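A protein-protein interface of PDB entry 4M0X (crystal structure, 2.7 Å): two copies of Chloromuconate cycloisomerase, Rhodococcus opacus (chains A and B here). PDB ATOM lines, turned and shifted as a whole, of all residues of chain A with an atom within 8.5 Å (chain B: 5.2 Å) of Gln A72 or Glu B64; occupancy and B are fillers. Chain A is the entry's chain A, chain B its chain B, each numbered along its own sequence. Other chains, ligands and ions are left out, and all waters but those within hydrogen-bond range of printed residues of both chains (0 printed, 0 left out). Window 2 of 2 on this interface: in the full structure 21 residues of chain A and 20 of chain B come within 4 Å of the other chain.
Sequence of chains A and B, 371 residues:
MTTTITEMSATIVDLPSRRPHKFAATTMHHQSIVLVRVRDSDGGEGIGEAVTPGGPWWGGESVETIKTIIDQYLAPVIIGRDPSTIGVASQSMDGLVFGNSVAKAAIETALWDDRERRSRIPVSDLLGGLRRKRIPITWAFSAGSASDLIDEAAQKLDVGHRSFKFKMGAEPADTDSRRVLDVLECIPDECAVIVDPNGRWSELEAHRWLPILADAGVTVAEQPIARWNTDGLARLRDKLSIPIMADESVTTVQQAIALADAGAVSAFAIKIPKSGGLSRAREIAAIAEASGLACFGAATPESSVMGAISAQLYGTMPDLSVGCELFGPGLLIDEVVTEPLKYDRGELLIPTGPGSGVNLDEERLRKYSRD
The side-chain hydroxyl (OH) of Tyr A73 sits at hydrogen-bond distance from the side-chain carboxylate (OE1) of Glu B64, at 2.5 Å.
NE2 of Gln A72 lies within hydrogen-bond range of OE1 of Glu B64, 3.0 Å away.
O of Glu A64 lies within hydrogen-bond range of OG1 of Thr A68, 3.5 Å away.
The side-chain hydroxyl (OG) of Ser B62 sits at hydrogen-bond distance from the side-chain hydroxyl (OG1) of Thr B65, 2.9 Å away.
The side-chain hydroxyl (OH) of Tyr A73 sits at hydrogen-bond distance from the side-chain amide nitrogen (NE2) of Gln A72.
N of Leu A74 is in hydrogen-bond range of O of Ile A69, at 2.8 Å.
The side-chain carboxylate of Glu B64 is in salt-bridge range of the guanidinium group of Arg B370, 2.4 Å away.
OG1 of Thr B68 sits at hydrogen-bond distance from O of Glu B64, 3.2 Å away.
Thr B68 touches Glu A64.
Thr B65 touches Thr A65 (O to CG2, 3.8 Å).
Glu B64 touches Thr A68.
Ile A69 touches Thr B65.
Tyr A73 touches Ser B62.
Gln A72 touches one residue of chain B.
Glu B64 touches just these residues of chain A: Thr A68, Gln A72 and Tyr A73.
Thr B65 touches just these residues of chain A: Thr A65 (3.8 Å) and Ile A69 (3.8 Å).
Of the printed residues of chain B, Glu A64 touches Thr B68 (3.98 Å).
Printed residues of chain B within 4 Å of Thr A68: Glu B64.
Printed residues of chain B within 4 Å of Ile A69: Thr B65 (3.8 Å).
Of the 9 printed residues of chain B, 4 touch a printed residue of chain A.
Of the 18 printed residues of chain A, 6 touch a printed residue of chain B.
Printed residues of chain A that touch a printed residue of chain B: Glu A64, Thr A65, Thr A68, Ile A69, Gln A72 and Tyr A73.
Hydrophobic or aromatic side chains of chain A that line the printed part of chain B: Ile A69 and Tyr A73.
Among the printed residues, no Asp or Glu carboxylate lies within 4 Å of a Lys or Arg side-chain nitrogen of the other chain.
Glu A64 touches Thr B68, and with the chains exchanged Thr A68 touches Glu B64.
Thr B65 touches its own counterpart, Thr A65.
Positions printed for both chains: 64, 65, 66, 67 and 68.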
ATOM      1  N   MET A   8       5.427 -26.734   7.418  1.00  0.00           N
ATOM      2  CA  MET A   8       6.117 -25.621   6.811  1.00  0.00           C
ATOM      3  C   MET A   8       7.407 -26.176   6.249  1.00  0.00           C
ATOM      4  O   MET A   8       8.227 -26.715   6.991  1.00  0.00           O
ATOM      5  CB  MET A   8       6.402 -24.521   7.830  1.00  0.00           C
ATOM      6  CG  MET A   8       7.310 -23.421   7.288  1.00  0.00           C
ATOM      7  SD  MET A   8       7.589 -22.071   8.444  1.00  0.00           S
ATOM      8  CE  MET A   8       8.527 -22.844   9.760  1.00  0.00           C
ATOM      9  N   ALA A  10      10.860 -25.335   3.626  1.00  0.00           N
ATOM     10  CA  ALA A  10      11.713 -24.288   3.080  1.00  0.00           C
ATOM     11  C   ALA A  10      12.690 -24.883   2.035  1.00  0.00           C
ATOM     12  O   ALA A  10      13.660 -25.581   2.384  1.00  0.00           O
ATOM     13  CB  ALA A  10      12.459 -23.585   4.205  1.00  0.00           C
ATOM     14  N   GLU A  64      21.289 -20.708   1.833  1.00  0.00           N
ATOM     15  CA  GLU A  64      21.653 -21.946   2.502  1.00  0.00           C
ATOM     16  C   GLU A  64      21.394 -21.822   3.988  1.00  0.00           C
ATOM     17  O   GLU A  64      20.821 -22.718   4.577  1.00  0.00           O
ATOM     18  CB  GLU A  64      23.117 -22.327   2.233  1.00  0.00           C
ATOM     19  CG  GLU A  64      23.426 -22.761   0.802  1.00  0.00           C
ATOM     20  CD  GLU A  64      23.600 -21.588  -0.144  1.00  0.00           C
ATOM     21  OE1 GLU A  64      23.437 -20.421   0.304  1.00  0.00           O
ATOM     22  OE2 GLU A  64      23.900 -21.820  -1.339  1.00  0.00           O
ATOM     23  N   THR A  65      21.780 -20.702   4.586  1.00  0.00           N
ATOM     24  CA  THR A  65      21.600 -20.515   6.024  1.00  0.00           C
ATOM     25  C   THR A  65      20.187 -20.109   6.364  1.00  0.00           C
ATOM     26  O   THR A  65      19.714 -20.365   7.487  1.00  0.00           O
ATOM     27  CB  THR A  65      22.548 -19.471   6.609  1.00  0.00           C
ATOM     28  OG1 THR A  65      22.211 -18.179   6.083  1.00  0.00           O
ATOM     29  CG2 THR A  65      23.972 -19.819   6.284  1.00  0.00           C
ATOM     30  N   ILE A  66      19.505 -19.486   5.402  1.00  0.00           N
ATOM     31  CA  ILE A  66      18.105 -19.121   5.631  1.00  0.00           C
ATOM     32  C   ILE A  66      17.309 -20.384   5.871  1.00  0.00           C
ATOM     33  O   ILE A  66      16.621 -20.489   6.892  1.00  0.00           O
ATOM     34  CB  ILE A  66      17.481 -18.289   4.495  1.00  0.00           C
ATOM     35  CG1 ILE A  66      17.879 -16.829   4.606  1.00  0.00           C
ATOM     36  CG2 ILE A  66      15.965 -18.381   4.510  1.00  0.00           C
ATOM     37  CD1 ILE A  66      17.852 -16.170   3.240  1.00  0.00           C
ATOM     38  N   LYS A  67      17.447 -21.356   4.969  1.00  0.00           N
ATOM     39  CA  LYS A  67      16.730 -22.617   5.124  1.00  0.00           C
ATOM     40  C   LYS A  67      16.923 -23.160   6.543  1.00  0.00           C
ATOM     41  O   LYS A  67      15.951 -23.455   7.236  1.00  0.00           O
ATOM     42  CB  LYS A  67      17.178 -23.654   4.103  1.00  0.00           C
ATOM     43  CG  LYS A  67      16.495 -24.994   4.310  1.00  0.00           C
ATOM     44  CD  LYS A  67      16.868 -26.021   3.251  1.00  0.00           C
ATOM     45  CE  LYS A  67      16.479 -27.445   3.651  1.00  0.00           C
ATOM     46  NZ  LYS A  67      15.011 -27.648   3.753  1.00  0.00           N
ATOM     47  N   THR A  68      18.177 -23.244   6.984  1.00  0.00           N
ATOM     48  CA  THR A  68      18.483 -23.828   8.274  1.00  0.00           C
ATOM     49  C   THR A  68      17.822 -23.112   9.434  1.00  0.00           C
ATOM     50  O   THR A  68      17.318 -23.769  10.332  1.00  0.00           O
ATOM     51  CB  THR A  68      19.987 -23.901   8.481  1.00  0.00           C
ATOM     52  OG1 THR A  68      20.520 -24.667   7.413  1.00  0.00           O
ATOM     53  CG2 THR A  68      20.330 -24.605   9.794  1.00  0.00           C
ATOM     54  N   ILE A  69      17.811 -21.777   9.402  1.00  0.00           N
ATOM     55  CA  ILE A  69      17.236 -20.963  10.486  1.00  0.00           C
ATOM     56  C   ILE A  69      15.745 -21.185  10.525  1.00  0.00           C
ATOM     57  O   ILE A  69      15.141 -21.344  11.597  1.00  0.00           O
ATOM     58  CB  ILE A  69      17.556 -19.465  10.298  1.00  0.00           C
ATOM     59  CG1 ILE A  69      19.003 -19.164  10.690  1.00  0.00           C
ATOM     60  CG2 ILE A  69      16.637 -18.588  11.111  1.00  0.00           C
ATOM     61  CD1 ILE A  69      19.321 -19.438  12.150  1.00  0.00           C
ATOM     62  N   ILE A  70      15.161 -21.232   9.338  1.00  0.00           N
ATOM     63  CA  ILE A  70      13.749 -21.525   9.220  1.00  0.00           C
ATOM     64  C   ILE A  70      13.450 -22.939   9.744  1.00  0.00           C
ATOM     65  O   ILE A  70      12.674 -23.082  10.702  1.00  0.00           O
ATOM     66  CB  ILE A  70      13.246 -21.300   7.790  1.00  0.00           C
ATOM     67  CG1 ILE A  70      13.243 -19.792   7.490  1.00  0.00           C
ATOM     68  CG2 ILE A  70      11.854 -21.857   7.618  1.00  0.00           C
ATOM     69  CD1 ILE A  70      13.096 -19.423   6.026  1.00  0.00           C
ATOM     70  N   ASP A  71      14.080 -23.959   9.140  1.00  0.00           N
ATOM     71  CA  ASP A  71      13.820 -25.371   9.508  1.00  0.00           C
ATOM     72  C   ASP A  71      14.078 -25.576  10.977  1.00  0.00           C
ATOM     73  O   ASP A  71      13.219 -26.102  11.648  1.00  0.00           O
ATOM     74  CB  ASP A  71      14.632 -26.393   8.698  1.00  0.00           C
ATOM     75  CG  ASP A  71      14.101 -26.591   7.299  1.00  0.00           C
ATOM     76  OD1 ASP A  71      12.949 -26.208   7.012  1.00  0.00           O
ATOM     77  OD2 ASP A  71      14.839 -27.113   6.448  1.00  0.00           O
ATOM     78  N   GLN A  72      15.222 -25.120  11.490  1.00  0.00           N
ATOM     79  CA  GLN A  72      15.618 -25.530  12.824  1.00  0.00           C
ATOM     80  C   GLN A  72      15.174 -24.607  13.941  1.00  0.00           C
ATOM     81  O   GLN A  72      14.704 -25.108  14.986  1.00  0.00           O
ATOM     82  CB  GLN A  72      17.113 -25.784  12.906  1.00  0.00           C
ATOM     83  CG  GLN A  72      17.596 -26.238  14.275  1.00  0.00           C
ATOM     84  CD  GLN A  72      19.086 -26.549  14.302  1.00  0.00           C
ATOM     85  OE1 GLN A  72      19.740 -26.672  13.251  1.00  0.00           O
ATOM     86  NE2 GLN A  72      19.630 -26.694  15.514  1.00  0.00           N
ATOM     87  N   TYR A  73      15.336 -23.287  13.761  1.00  0.00           N
ATOM     88  CA  TYR A  73      15.102 -22.370  14.897  1.00  0.00           C
ATOM     89  C   TYR A  73      13.824 -21.577  14.852  1.00  0.00           C
ATOM     90  O   TYR A  73      13.334 -21.133  15.892  1.00  0.00           O
ATOM     91  CB  TYR A  73      16.270 -21.421  15.132  1.00  0.00           C
ATOM     92  CG  TYR A  73      17.555 -22.120  15.465  1.00  0.00           C
ATOM     93  CD1 TYR A  73      17.894 -22.409  16.786  1.00  0.00           C
ATOM     94  CD2 TYR A  73      18.433 -22.493  14.454  1.00  0.00           C
ATOM     95  CE1 TYR A  73      19.076 -23.051  17.095  1.00  0.00           C
ATOM     96  CE2 TYR A  73      19.618 -23.138  14.744  1.00  0.00           C
ATOM     97  CZ  TYR A  73      19.936 -23.405  16.061  1.00  0.00           C
ATOM     98  OH  TYR A  73      21.124 -24.026  16.319  1.00  0.00           O
ATOM     99  N   LEU A  74      13.294 -21.370  13.655  1.00  0.00           N
ATOM    100  CA  LEU A  74      12.061 -20.610  13.532  1.00  0.00           C
ATOM    101  C   LEU A  74      10.844 -21.513  13.586  1.00  0.00           C
ATOM    102  O   LEU A  74       9.859 -21.159  14.211  1.00  0.00           O
ATOM    103  CB  LEU A  74      12.085 -19.738  12.259  1.00  0.00           C
ATOM    104  CG  LEU A  74      13.027 -18.510  12.305  1.00  0.00           C
ATOM    105  CD1 LEU A  74      12.913 -17.597  11.088  1.00  0.00           C
ATOM    106  CD2 LEU A  74      12.797 -17.717  13.571  1.00  0.00           C
ATOM    107  N   ALA A  75      10.946 -22.694  12.964  1.00  0.00           N
ATOM    108  CA  ALA A  75       9.819 -23.611  12.745  1.00  0.00           C
ATOM    109  C   ALA A  75       8.964 -23.845  13.978  1.00  0.00           C
ATOM    110  O   ALA A  75       7.745 -23.750  13.883  1.00  0.00           O
ATOM    111  CB  ALA A  75      10.297 -24.941  12.185  1.00  0.00           C
ATOM    112  N   PRO A  76       9.606 -24.174  15.124  1.00  0.00           N
ATOM    113  CA  PRO A  76       9.046 -24.408  16.453  1.00  0.00           C
ATOM    114  C   PRO A  76       8.050 -23.391  16.979  1.00  0.00           C
ATOM    115  O   PRO A  76       7.203 -23.761  17.802  1.00  0.00           O
ATOM    116  CB  PRO A  76      10.282 -24.397  17.361  1.00  0.00           C
ATOM    117  CG  PRO A  76      11.451 -24.078  16.473  1.00  0.00           C
ATOM    118  CD  PRO A  76      11.033 -24.532  15.124  1.00  0.00           C
ATOM    119  N   VAL A  77       8.131 -22.130  16.570  1.00  0.00           N
ATOM    120  CA  VAL A  77       7.030 -21.239  16.937  1.00  0.00           C
ATOM    121  C   VAL A  77       5.962 -21.082  15.845  1.00  0.00           C
ATOM    122  O   VAL A  77       5.045 -20.281  15.997  1.00  0.00           O
ATOM    123  CB  VAL A  77       7.474 -19.871  17.524  1.00  0.00           C
ATOM    124  CG1 VAL A  77       7.876 -20.019  18.990  1.00  0.00           C
ATOM    125  CG2 VAL A  77       8.578 -19.223  16.701  1.00  0.00           C
ATOM    126  N   LEU A  96      13.344 -15.983  19.692  1.00  0.00           N
ATOM    127  CA  LEU A  96      14.326 -17.081  19.460  1.00  0.00           C
ATOM    128  C   LEU A  96      15.514 -16.697  18.595  1.00  0.00           C
ATOM    129  O   LEU A  96      16.615 -17.198  18.815  1.00  0.00           O
ATOM    130  CB  LEU A  96      13.694 -18.345  18.842  1.00  0.00           C
ATOM    131  CG  LEU A  96      12.439 -18.901  19.493  1.00  0.00           C
ATOM    132  CD1 LEU A  96      12.025 -20.198  18.833  1.00  0.00           C
ATOM    133  CD2 LEU A  96      12.651 -19.072  20.994  1.00  0.00           C
ATOM    134  N   VAL A  97      15.301 -15.853  17.585  1.00  0.00           N
ATOM    135  CA  VAL A  97      16.439 -15.488  16.743  1.00  0.00           C
ATOM    136  C   VAL A  97      16.602 -14.005  16.528  1.00  0.00           C
ATOM    137  O   VAL A  97      15.699 -13.315  16.053  1.00  0.00           O
ATOM    138  CB  VAL A  97      16.594 -16.350  15.439  1.00  0.00           C
ATOM    139  CG1 VAL A  97      15.303 -17.002  15.036  1.00  0.00           C
ATOM    140  CG2 VAL A  97      17.170 -15.555  14.273  1.00  0.00           C
ATOM    141  N   ILE B  12      31.471 -28.950  13.728  1.00  0.00           N
ATOM    142  CA  ILE B  12      30.576 -28.751  14.864  1.00  0.00           C
ATOM    143  C   ILE B  12      30.859 -29.766  15.978  1.00  0.00           C
ATOM    144  O   ILE B  12      30.986 -30.953  15.744  1.00  0.00           O
ATOM    145  CB  ILE B  12      29.098 -28.834  14.456  1.00  0.00           C
ATOM    146  CG1 ILE B  12      28.776 -27.772  13.392  1.00  0.00           C
ATOM    147  CG2 ILE B  12      28.202 -28.692  15.689  1.00  0.00           C
ATOM    148  CD1 ILE B  12      27.568 -28.107  12.531  1.00  0.00           C
ATOM    149  N   SER B  62      24.290 -19.400  14.642  1.00  0.00           N
ATOM    150  CA  SER B  62      24.220 -20.736  15.200  1.00  0.00           C
ATOM    151  C   SER B  62      25.322 -21.618  14.630  1.00  0.00           C
ATOM    152  O   SER B  62      25.783 -21.410  13.498  1.00  0.00           O
ATOM    153  CB  SER B  62      22.846 -21.344  14.908  1.00  0.00           C
ATOM    154  OG  SER B  62      22.679 -21.537  13.526  1.00  0.00           O
ATOM    155  N   VAL B  63      25.734 -22.624  15.385  1.00  0.00           N
ATOM    156  CA  VAL B  63      26.794 -23.506  14.891  1.00  0.00           C
ATOM    157  C   VAL B  63      26.509 -24.075  13.491  1.00  0.00           C
ATOM    158  O   VAL B  63      27.423 -24.174  12.661  1.00  0.00           O
ATOM    159  CB  VAL B  63      27.156 -24.635  15.884  1.00  0.00           C
ATOM    160  CG1 VAL B  63      27.704 -24.057  17.178  1.00  0.00           C
ATOM    161  CG2 VAL B  63      25.968 -25.553  16.135  1.00  0.00           C
ATOM    162  N   GLU B  64      25.250 -24.442  13.240  1.00  0.00           N
ATOM    163  CA  GLU B  64      24.867 -25.004  11.940  1.00  0.00           C
ATOM    164  C   GLU B  64      25.069 -23.976  10.823  1.00  0.00           C
ATOM    165  O   GLU B  64      25.624 -24.297   9.777  1.00  0.00           O
ATOM    166  CB  GLU B  64      23.405 -25.476  11.945  1.00  0.00           C
ATOM    167  CG  GLU B  64      23.103 -26.733  12.762  1.00  0.00           C
ATOM    168  CD  GLU B  64      22.760 -26.450  14.221  1.00  0.00           C
ATOM    169  OE1 GLU B  64      22.170 -25.392  14.528  1.00  0.00           O
ATOM    170  OE2 GLU B  64      23.071 -27.298  15.080  1.00  0.00           O
ATOM    171  N   THR B  65      24.632 -22.737  11.056  1.00  0.00           N
ATOM    172  CA  THR B  65      24.729 -21.701  10.035  1.00  0.00           C
ATOM    173  C   THR B  65      26.140 -21.163   9.924  1.00  0.00           C
ATOM    174  O   THR B  65      26.572 -20.782   8.836  1.00  0.00           O
ATOM    175  CB  THR B  65      23.739 -20.548  10.271  1.00  0.00           C
ATOM    176  OG1 THR B  65      23.999 -19.927  11.539  1.00  0.00           O
ATOM    177  CG2 THR B  65      22.270 -21.061  10.228  1.00  0.00           C
ATOM    178  N   ILE B  66      26.860 -21.151  11.041  1.00  0.00           N
ATOM    179  CA  ILE B  66      28.272 -20.732  11.084  1.00  0.00           C
ATOM    180  C   ILE B  66      29.125 -21.652  10.213  1.00  0.00           C
ATOM    181  O   ILE B  66      29.957 -21.197   9.404  1.00  0.00           O
ATOM    182  CB  ILE B  66      28.803 -20.714  12.547  1.00  0.00           C
ATOM    183  CG1 ILE B  66      28.430 -19.413  13.276  1.00  0.00           C
ATOM    184  CG2 ILE B  66      30.301 -20.929  12.627  1.00  0.00           C
ATOM    185  CD1 ILE B  66      28.247 -19.610  14.773  1.00  0.00           C
ATOM    186  N   LYS B  67      28.908 -22.956  10.374  1.00  0.00           N
ATOM    187  CA  LYS B  67      29.664 -23.933   9.615  1.00  0.00           C
ATOM    188  C   LYS B  67      29.561 -23.626   8.120  1.00  0.00           C
ATOM    189  O   LYS B  67      30.570 -23.552   7.433  1.00  0.00           O
ATOM    190  CB  LYS B  67      29.201 -25.355   9.926  1.00  0.00           C
ATOM    191  CG  LYS B  67      29.953 -26.377   9.090  1.00  0.00           C
ATOM    192  CD  LYS B  67      29.796 -27.812   9.551  1.00  0.00           C
ATOM    193  CE  LYS B  67      30.299 -28.736   8.450  1.00  0.00           C
ATOM    194  NZ  LYS B  67      31.718 -28.506   8.036  1.00  0.00           N
ATOM    195  N   THR B  68      28.334 -23.404   7.648  1.00  0.00           N
ATOM    196  CA  THR B  68      28.087 -23.093   6.252  1.00  0.00           C
ATOM    197  C   THR B  68      28.792 -21.835   5.768  1.00  0.00           C
ATOM    198  O   THR B  68      29.457 -21.856   4.702  1.00  0.00           O
ATOM    199  CB  THR B  68      26.606 -22.888   5.996  1.00  0.00           C
ATOM    200  OG1 THR B  68      25.904 -23.954   6.613  1.00  0.00           O
ATOM    201  CG2 THR B  68      26.341 -22.897   4.492  1.00  0.00           C
ATOM    202  N   ARG B 370      29.973 -33.648  16.231  1.00  0.00           N
ATOM    203  CA  ARG B 370      28.649 -34.058  15.795  1.00  0.00           C
ATOM    204  C   ARG B 370      28.789 -34.492  14.339  1.00  0.00           C
ATOM    205  O   ARG B 370      28.344 -35.572  13.962  1.00  0.00           O
ATOM    206  CB  ARG B 370      27.682 -32.891  15.927  1.00  0.00           C
ATOM    207  CG  ARG B 370      26.244 -33.183  15.524  1.00  0.00           C
ATOM    208  CD  ARG B 370      25.533 -31.895  15.200  1.00  0.00           C
ATOM    209  NE  ARG B 370      25.580 -30.970  16.333  1.00  0.00           N
ATOM    210  CZ  ARG B 370      24.859 -29.846  16.406  1.00  0.00           C
ATOM    211  NH1 ARG B 370      24.058 -29.512  15.394  1.00  0.00           N
ATOM    212  NH2 ARG B 370      24.937 -29.042  17.473  1.00  0.00           N
